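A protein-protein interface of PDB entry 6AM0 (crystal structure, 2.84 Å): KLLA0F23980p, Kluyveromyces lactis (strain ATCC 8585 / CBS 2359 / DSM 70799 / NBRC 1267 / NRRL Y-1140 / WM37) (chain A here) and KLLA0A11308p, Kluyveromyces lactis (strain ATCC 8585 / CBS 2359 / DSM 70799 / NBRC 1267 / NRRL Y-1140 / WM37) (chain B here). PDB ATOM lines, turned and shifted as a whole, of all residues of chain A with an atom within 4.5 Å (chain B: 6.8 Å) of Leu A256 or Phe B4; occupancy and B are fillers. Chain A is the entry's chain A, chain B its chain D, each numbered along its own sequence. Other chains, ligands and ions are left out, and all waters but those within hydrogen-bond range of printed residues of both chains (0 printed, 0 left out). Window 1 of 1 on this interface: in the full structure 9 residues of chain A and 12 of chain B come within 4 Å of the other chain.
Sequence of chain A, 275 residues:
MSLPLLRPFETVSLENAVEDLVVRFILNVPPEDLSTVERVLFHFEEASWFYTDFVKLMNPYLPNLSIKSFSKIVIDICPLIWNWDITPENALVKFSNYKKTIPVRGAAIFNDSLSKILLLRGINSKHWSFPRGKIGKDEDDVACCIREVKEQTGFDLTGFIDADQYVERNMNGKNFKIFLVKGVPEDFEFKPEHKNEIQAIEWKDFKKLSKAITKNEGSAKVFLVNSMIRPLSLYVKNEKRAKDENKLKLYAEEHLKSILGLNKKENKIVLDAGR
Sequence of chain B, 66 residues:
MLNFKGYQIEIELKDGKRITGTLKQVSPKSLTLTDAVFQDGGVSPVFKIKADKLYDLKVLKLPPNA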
ATOM      1  N   ALA A 252      -1.486 -22.008  28.561  1.00  0.00           N
ATOM      2  CA  ALA A 252      -0.505 -20.952  28.354  1.00  0.00           C
ATOM      3  C   ALA A 252       0.177 -21.083  26.998  1.00  0.00           C
ATOM      4  O   ALA A 252      -0.026 -20.230  26.133  1.00  0.00           O
ATOM      5  CB  ALA A 252       0.538 -20.956  29.470  1.00  0.00           C
ATOM      6  N   GLU A 253       0.961 -22.149  26.791  1.00  0.00           N
ATOM      7  CA  GLU A 253       1.775 -22.241  25.578  1.00  0.00           C
ATOM      8  C   GLU A 253       0.942 -22.077  24.314  1.00  0.00           C
ATOM      9  O   GLU A 253       1.388 -21.446  23.345  1.00  0.00           O
ATOM     10  CB  GLU A 253       2.538 -23.567  25.536  1.00  0.00           C
ATOM     11  CG  GLU A 253       1.742 -24.785  25.955  1.00  0.00           C
ATOM     12  CD  GLU A 253       2.629 -25.984  26.240  1.00  0.00           C
ATOM     13  OE1 GLU A 253       3.464 -26.326  25.375  1.00  0.00           O
ATOM     14  OE2 GLU A 253       2.504 -26.573  27.335  1.00  0.00           O
ATOM     15  N   GLU A 254      -0.275 -22.625  24.305  1.00  0.00           N
ATOM     16  CA  GLU A 254      -1.124 -22.429  23.135  1.00  0.00           C
ATOM     17  C   GLU A 254      -1.491 -20.958  22.966  1.00  0.00           C
ATOM     18  O   GLU A 254      -1.415 -20.412  21.856  1.00  0.00           O
ATOM     19  CB  GLU A 254      -2.376 -23.301  23.239  1.00  0.00           C
ATOM     20  CG  GLU A 254      -3.121 -23.453  21.924  1.00  0.00           C
ATOM     21  CD  GLU A 254      -3.937 -24.728  21.859  1.00  0.00           C
ATOM     22  OE1 GLU A 254      -4.740 -24.871  20.911  1.00  0.00           O
ATOM     23  OE2 GLU A 254      -3.774 -25.588  22.752  1.00  0.00           O
ATOM     24  N   HIS A 255      -1.852 -20.287  24.065  1.00  0.00           N
ATOM     25  CA  HIS A 255      -2.218 -18.876  23.968  1.00  0.00           C
ATOM     26  C   HIS A 255      -1.038 -18.005  23.543  1.00  0.00           C
ATOM     27  O   HIS A 255      -1.205 -17.083  22.738  1.00  0.00           O
ATOM     28  CB  HIS A 255      -2.796 -18.393  25.294  1.00  0.00           C
ATOM     29  CG  HIS A 255      -4.257 -18.669  25.444  1.00  0.00           C
ATOM     30  ND1 HIS A 255      -5.091 -18.858  24.363  1.00  0.00           N
ATOM     31  CD2 HIS A 255      -5.033 -18.796  26.544  1.00  0.00           C
ATOM     32  CE1 HIS A 255      -6.320 -19.085  24.792  1.00  0.00           C
ATOM     33  NE2 HIS A 255      -6.312 -19.052  26.112  1.00  0.00           N
ATOM     34  N   LEU A 256       0.158 -18.265  24.080  1.00  0.00           N
ATOM     35  CA  LEU A 256       1.330 -17.500  23.665  1.00  0.00           C
ATOM     36  C   LEU A 256       1.622 -17.717  22.188  1.00  0.00           C
ATOM     37  O   LEU A 256       1.900 -16.762  21.452  1.00  0.00           O
ATOM     38  CB  LEU A 256       2.550 -17.876  24.509  1.00  0.00           C
ATOM     39  CG  LEU A 256       2.738 -17.201  25.868  1.00  0.00           C
ATOM     40  CD1 LEU A 256       1.934 -17.912  26.935  1.00  0.00           C
ATOM     41  CD2 LEU A 256       4.211 -17.167  26.242  1.00  0.00           C
ATOM     42  N   LYS A 257       1.560 -18.970  21.729  1.00  0.00           N
ATOM     43  CA  LYS A 257       1.734 -19.214  20.302  1.00  0.00           C
ATOM     44  C   LYS A 257       0.606 -18.617  19.470  1.00  0.00           C
ATOM     45  O   LYS A 257       0.749 -18.520  18.246  1.00  0.00           O
ATOM     46  CB  LYS A 257       1.856 -20.713  20.023  1.00  0.00           C
ATOM     47  CG  LYS A 257       3.291 -21.175  19.828  1.00  0.00           C
ATOM     48  CD  LYS A 257       3.353 -22.595  19.289  1.00  0.00           C
ATOM     49  CE  LYS A 257       4.789 -23.012  19.005  1.00  0.00           C
ATOM     50  NZ  LYS A 257       4.886 -24.399  18.469  1.00  0.00           N
ATOM     51  N   SER A 258      -0.503 -18.219  20.099  1.00  0.00           N
ATOM     52  CA  SER A 258      -1.513 -17.434  19.395  1.00  0.00           C
ATOM     53  C   SER A 258      -1.144 -15.955  19.347  1.00  0.00           C
ATOM     54  O   SER A 258      -1.325 -15.304  18.312  1.00  0.00           O
ATOM     55  CB  SER A 258      -2.878 -17.612  20.057  1.00  0.00           C
ATOM     56  OG  SER A 258      -3.821 -16.698  19.523  1.00  0.00           O
ATOM     57  N   ILE A 259      -0.641 -15.407  20.457  1.00  0.00           N
ATOM     58  CA  ILE A 259      -0.256 -13.998  20.491  1.00  0.00           C
ATOM     59  C   ILE A 259       0.833 -13.725  19.463  1.00  0.00           C
ATOM     60  O   ILE A 259       0.768 -12.753  18.702  1.00  0.00           O
ATOM     61  CB  ILE A 259       0.188 -13.598  21.909  1.00  0.00           C
ATOM     62  CG1 ILE A 259      -1.008 -13.619  22.861  1.00  0.00           C
ATOM     63  CG2 ILE A 259       0.838 -12.225  21.899  1.00  0.00           C
ATOM     64  CD1 ILE A 259      -0.679 -13.184  24.267  1.00  0.00           C
ATOM     65  N   LEU A 260       1.842 -14.585  19.418  1.00  0.00           N
ATOM     66  CA  LEU A 260       2.878 -14.497  18.404  1.00  0.00           C
ATOM     67  C   LEU A 260       2.437 -15.302  17.183  1.00  0.00           C
ATOM     68  O   LEU A 260       1.292 -15.753  17.092  1.00  0.00           O
ATOM     69  CB  LEU A 260       4.217 -14.978  18.963  1.00  0.00           C
ATOM     70  CG  LEU A 260       4.882 -14.173  20.086  1.00  0.00           C
ATOM     71  CD1 LEU A 260       4.183 -14.348  21.428  1.00  0.00           C
ATOM     72  CD2 LEU A 260       6.341 -14.561  20.205  1.00  0.00           C
ATOM     73  N   MET B   1      -5.161 -13.817  33.228  1.00  0.00           N
ATOM     74  CA  MET B   1      -5.318 -12.555  32.514  1.00  0.00           C
ATOM     75  C   MET B   1      -4.614 -12.661  31.162  1.00  0.00           C
ATOM     76  O   MET B   1      -3.978 -13.675  30.865  1.00  0.00           O
ATOM     77  CB  MET B   1      -4.758 -11.388  33.348  1.00  0.00           C
ATOM     78  CG  MET B   1      -5.113  -9.973  32.857  1.00  0.00           C
ATOM     79  SD  MET B   1      -4.123  -8.668  33.628  1.00  0.00           S
ATOM     80  CE  MET B   1      -3.792  -7.590  32.231  1.00  0.00           C
ATOM     81  N   LEU B   2      -4.748 -11.615  30.340  1.00  0.00           N
ATOM     82  CA  LEU B   2      -4.043 -11.565  29.065  1.00  0.00           C
ATOM     83  C   LEU B   2      -2.538 -11.686  29.252  1.00  0.00           C
ATOM     84  O   LEU B   2      -1.827 -12.101  28.328  1.00  0.00           O
ATOM     85  CB  LEU B   2      -4.371 -10.263  28.339  1.00  0.00           C
ATOM     86  CG  LEU B   2      -4.085 -10.351  26.847  1.00  0.00           C
ATOM     87  CD1 LEU B   2      -4.918 -11.491  26.297  1.00  0.00           C
ATOM     88  CD2 LEU B   2      -4.382  -9.037  26.146  1.00  0.00           C
ATOM     89  N   ASN B   3      -2.039 -11.315  30.425  1.00  0.00           N
ATOM     90  CA  ASN B   3      -0.620 -11.385  30.724  1.00  0.00           C
ATOM     91  C   ASN B   3      -0.265 -12.778  31.226  1.00  0.00           C
ATOM     92  O   ASN B   3      -1.020 -13.399  31.979  1.00  0.00           O
ATOM     93  CB  ASN B   3      -0.221 -10.325  31.755  1.00  0.00           C
ATOM     94  CG  ASN B   3      -0.557 -10.728  33.179  1.00  0.00           C
ATOM     95  OD1 ASN B   3      -1.667 -11.170  33.470  1.00  0.00           O
ATOM     96  ND2 ASN B   3       0.411 -10.578  34.076  1.00  0.00           N
ATOM     97  N   PHE B   4       0.879 -13.269  30.777  1.00  0.00           N
ATOM     98  CA  PHE B   4       1.438 -14.535  31.228  1.00  0.00           C
ATOM     99  C   PHE B   4       2.750 -14.279  31.952  1.00  0.00           C
ATOM    100  O   PHE B   4       3.662 -15.105  31.940  1.00  0.00           O
ATOM    101  CB  PHE B   4       1.615 -15.487  30.048  1.00  0.00           C
ATOM    102  CG  PHE B   4       0.321 -15.874  29.391  1.00  0.00           C
ATOM    103  CD1 PHE B   4      -0.588 -16.679  30.054  1.00  0.00           C
ATOM    104  CD2 PHE B   4      -0.003 -15.400  28.131  1.00  0.00           C
ATOM    105  CE1 PHE B   4      -1.783 -17.033  29.462  1.00  0.00           C
ATOM    106  CE2 PHE B   4      -1.201 -15.751  27.534  1.00  0.00           C
ATOM    107  CZ  PHE B   4      -2.092 -16.566  28.203  1.00  0.00           C
ATOM    108  N   LYS B   5       2.838 -13.111  32.579  1.00  0.00           N
ATOM    109  CA  LYS B   5       4.058 -12.689  33.247  1.00  0.00           C
ATOM    110  C   LYS B   5       4.361 -13.599  34.428  1.00  0.00           C
ATOM    111  O   LYS B   5       3.483 -13.902  35.241  1.00  0.00           O
ATOM    112  CB  LYS B   5       3.895 -11.240  33.698  1.00  0.00           C
ATOM    113  CG  LYS B   5       3.875 -10.289  32.513  1.00  0.00           C
ATOM    114  CD  LYS B   5       3.080  -9.026  32.798  1.00  0.00           C
ATOM    115  CE  LYS B   5       2.812  -8.260  31.511  1.00  0.00           C
ATOM    116  NZ  LYS B   5       2.384  -6.860  31.766  1.00  0.00           N
ATOM    117  N   GLY B   6       5.613 -14.042  34.508  1.00  0.00           N
ATOM    118  CA  GLY B   6       6.060 -14.976  35.516  1.00  0.00           C
ATOM    119  C   GLY B   6       6.190 -16.403  35.029  1.00  0.00           C
ATOM    120  O   GLY B   6       6.794 -17.225  35.730  1.00  0.00           O
ATOM    121  N   TYR B   7       5.636 -16.722  33.862  1.00  0.00           N
ATOM    122  CA  TYR B   7       5.765 -18.063  33.314  1.00  0.00           C
ATOM    123  C   TYR B   7       7.195 -18.311  32.846  1.00  0.00           C
ATOM    124  O   TYR B   7       7.840 -17.433  32.265  1.00  0.00           O
ATOM    125  CB  TYR B   7       4.784 -18.252  32.155  1.00  0.00           C
ATOM    126  CG  TYR B   7       3.365 -18.545  32.595  1.00  0.00           C
ATOM    127  CD1 TYR B   7       2.664 -17.639  33.380  1.00  0.00           C
ATOM    128  CD2 TYR B   7       2.719 -19.712  32.214  1.00  0.00           C
ATOM    129  CE1 TYR B   7       1.365 -17.890  33.785  1.00  0.00           C
ATOM    130  CE2 TYR B   7       1.417 -19.973  32.617  1.00  0.00           C
ATOM    131  CZ  TYR B   7       0.745 -19.057  33.400  1.00  0.00           C
ATOM    132  OH  TYR B   7      -0.547 -19.302  33.805  1.00  0.00           O
ATOM    133  N   GLN B   8       7.677 -19.531  33.075  1.00  0.00           N
ATOM    134  CA  GLN B   8       9.006 -19.941  32.639  1.00  0.00           C
ATOM    135  C   GLN B   8       8.944 -20.369  31.176  1.00  0.00           C
ATOM    136  O   GLN B   8       8.161 -21.256  30.820  1.00  0.00           O
ATOM    137  CB  GLN B   8       9.508 -21.075  33.528  1.00  0.00           C
ATOM    138  CG  GLN B   8      10.968 -21.470  33.362  1.00  0.00           C
ATOM    139  CD  GLN B   8      11.936 -20.316  33.553  1.00  0.00           C
ATOM    140  OE1 GLN B   8      11.584 -19.270  34.099  1.00  0.00           O
ATOM    141  NE2 GLN B   8      13.176 -20.514  33.125  1.00  0.00           N
ATOM    142  N   ILE B   9       9.772 -19.757  30.328  1.00  0.00           N
ATOM    143  CA  ILE B   9       9.630 -19.872  28.880  1.00  0.00           C
ATOM    144  C   ILE B   9      10.950 -20.328  28.273  1.00  0.00           C
ATOM    145  O   ILE B   9      12.029 -19.942  28.741  1.00  0.00           O
ATOM    146  CB  ILE B   9       9.175 -18.534  28.253  1.00  0.00           C
ATOM    147  CG1 ILE B   9       7.878 -18.044  28.902  1.00  0.00           C
ATOM    148  CG2 ILE B   9       8.992 -18.658  26.745  1.00  0.00           C
ATOM    149  CD1 ILE B   9       6.743 -19.039  28.832  1.00  0.00           C
ATOM    150  N   THR B  22      12.384 -15.772  32.016  1.00  0.00           N
ATOM    151  CA  THR B  22      11.091 -15.477  32.625  1.00  0.00           C
ATOM    152  C   THR B  22      10.376 -14.395  31.827  1.00  0.00           C
ATOM    153  O   THR B  22      10.982 -13.385  31.459  1.00  0.00           O
ATOM    154  CB  THR B  22      11.253 -15.060  34.088  1.00  0.00           C
ATOM    155  OG1 THR B  22      11.971 -13.822  34.163  1.00  0.00           O
ATOM    156  CG2 THR B  22      12.022 -16.121  34.855  1.00  0.00           C
ATOM    157  N   LEU B  23       9.091 -14.607  31.554  1.00  0.00           N
ATOM    158  CA  LEU B  23       8.347 -13.698  30.687  1.00  0.00           C
ATOM    159  C   LEU B  23       8.063 -12.384  31.410  1.00  0.00           C
ATOM    160  O   LEU B  23       7.373 -12.362  32.435  1.00  0.00           O
ATOM    161  CB  LEU B  23       7.052 -14.360  30.215  1.00  0.00           C
ATOM    162  CG  LEU B  23       5.978 -13.487  29.560  1.00  0.00           C
ATOM    163  CD1 LEU B  23       6.561 -12.706  28.406  1.00  0.00           C
ATOM    164  CD2 LEU B  23       4.833 -14.345  29.067  1.00  0.00           C
ATOM    165  N   LYS B  24       8.606 -11.291  30.870  1.00  0.00           N
ATOM    166  CA  LYS B  24       8.462  -9.940  31.401  1.00  0.00           C
ATOM    167  C   LYS B  24       7.228  -9.234  30.844  1.00  0.00           C
ATOM    168  O   LYS B  24       6.463  -8.629  31.601  1.00  0.00           O
ATOM    169  CB  LYS B  24       9.718  -9.127  31.070  1.00  0.00           C
ATOM    170  CG  LYS B  24       9.768  -7.736  31.665  1.00  0.00           C
ATOM    171  CD  LYS B  24       9.681  -7.750  33.171  1.00  0.00           C
ATOM    172  CE  LYS B  24      10.493  -6.603  33.752  1.00  0.00           C
ATOM    173  NZ  LYS B  24      11.894  -6.614  33.241  1.00  0.00           N
ATOM    174  N   VAL B  26       4.598  -9.477  26.893  1.00  0.00           N
ATOM    175  CA  VAL B  26       4.423 -10.016  25.549  1.00  0.00           C
ATOM    176  C   VAL B  26       3.358  -9.219  24.803  1.00  0.00           C
ATOM    177  O   VAL B  26       2.315  -8.865  25.365  1.00  0.00           O
ATOM    178  CB  VAL B  26       4.068 -11.519  25.590  1.00  0.00           C
ATOM    179  CG1 VAL B  26       2.838 -11.766  26.457  1.00  0.00           C
ATOM    180  CG2 VAL B  26       3.854 -12.060  24.185  1.00  0.00           C
ATOM    181  N   LEU B  31       8.617  -9.982  22.343  1.00  0.00           N
ATOM    182  CA  LEU B  31       8.622 -10.788  23.556  1.00  0.00           C
ATOM    183  C   LEU B  31       9.831 -10.404  24.396  1.00  0.00           C
ATOM    184  O   LEU B  31      10.952 -10.351  23.879  1.00  0.00           O
ATOM    185  CB  LEU B  31       8.667 -12.280  23.212  1.00  0.00           C
ATOM    186  CG  LEU B  31       9.175 -13.274  24.259  1.00  0.00           C
ATOM    187  CD1 LEU B  31       8.167 -13.485  25.376  1.00  0.00           C
ATOM    188  CD2 LEU B  31       9.529 -14.591  23.595  1.00  0.00           C
ATOM    189  N   LEU B  57       8.257 -22.180  20.413  1.00  0.00           N
ATOM    190  CA  LEU B  57       8.220 -21.731  21.798  1.00  0.00           C
ATOM    191  C   LEU B  57       7.508 -22.786  22.634  1.00  0.00           C
ATOM    192  O   LEU B  57       6.485 -23.330  22.208  1.00  0.00           O
ATOM    193  CB  LEU B  57       7.513 -20.370  21.909  1.00  0.00           C
ATOM    194  CG  LEU B  57       7.138 -19.768  23.266  1.00  0.00           C
ATOM    195  CD1 LEU B  57       7.239 -18.257  23.192  1.00  0.00           C
ATOM    196  CD2 LEU B  57       5.733 -20.170  23.693  1.00  0.00           C
ATOM    197  N   VAL B  59       6.713 -23.897  27.075  1.00  0.00           N
ATOM    198  CA  VAL B  59       6.659 -23.366  28.434  1.00  0.00           C
ATOM    199  C   VAL B  59       6.985 -24.474  29.429  1.00  0.00           C
ATOM    200  O   VAL B  59       6.552 -25.621  29.265  1.00  0.00           O
ATOM    201  CB  VAL B  59       5.277 -22.741  28.734  1.00  0.00           C
ATOM    202  CG1 VAL B  59       4.183 -23.757  28.532  1.00  0.00           C
ATOM    203  CG2 VAL B  59       5.220 -22.198  30.148  1.00  0.00           C
ATOM    204  N   PRO B  63       4.372 -19.443  37.380  1.00  0.00           N
ATOM    205  CA  PRO B  63       4.967 -18.467  38.297  1.00  0.00           C
ATOM    206  C   PRO B  63       4.853 -18.950  39.730  1.00  0.00           C
ATOM    207  O   PRO B  63       3.854 -19.586  40.096  1.00  0.00           O
ATOM    208  CB  PRO B  63       4.122 -17.205  38.064  1.00  0.00           C
ATOM    209  CG  PRO B  63       2.826 -17.718  37.535  1.00  0.00           C
ATOM    210  CD  PRO B  63       3.210 -18.879  36.670  1.00  0.00           C
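The backbone carbonyl oxygen (O) of Tyr B7 lies within hydrogen-bond range of the backbone NH (N) of Leu B23 (3.2 Å).
CB of Ala A252 touches CE2 of Tyr B7, 3.4 Å away. CB of Glu A253 touches CG1 of Val B59 (3.4 Å). Phe B4 touches His A255. Leu A256 touches Phe B4 (CD1 to CD2, 3.4 Å). O of Leu B57 touches CE of Lys A257, 3.6 Å away. Ile A259 touches Val B26 (CG2 to CG2, 3.8 Å). Val B26 touches Leu A260 (CG2 to CD1, 3.6 Å).
Of the printed residues of chain B, Ala A252 touches Tyr B7. Of the printed residues of chain B, Leu A256 touches Phe B4. Phe B4 touches just these residues of chain A: His A255 (3.5 Å) and Leu A256 (3.4 Å). Printed residues of chain A within 4 Å of Leu B57: Lys A257 (3.6 Å). Printed residues of chain A within 4 Å of Val B59: Glu A253 (3.4 Å). The nearest printed residue of chain B that does not touch Leu A256 is Leu B57 (4.01 Å). The nearest residue of chain A that does not touch Phe B4 is Ile A259 (4.2 Å). The nearest printed residue of chain A that does not touch Leu B57 is Leu A256 (4.01 Å).
Printed residues of chain A that touch a printed residue of chain B: Ala A252, Glu A253, His A255, Leu A256, Lys A257, Ile A259 and Leu A260. Hydrophobic or aromatic side chains of chain A that line the printed part of chain B: Ala A252, His A255, Leu A256, Ile A259 and Leu A260. Of the 17 printed residues of chain B, 5 touch a printed residue of chain A. Printed residues of chain B that touch a printed residue of chain A: Phe B4, Tyr B7, Val B26, Leu B57 and Val B59. Among the printed residues, no Asp or Glu carboxylate lies within 4 Å of a Lys or Arg side-chain nitrogen of the other chain.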
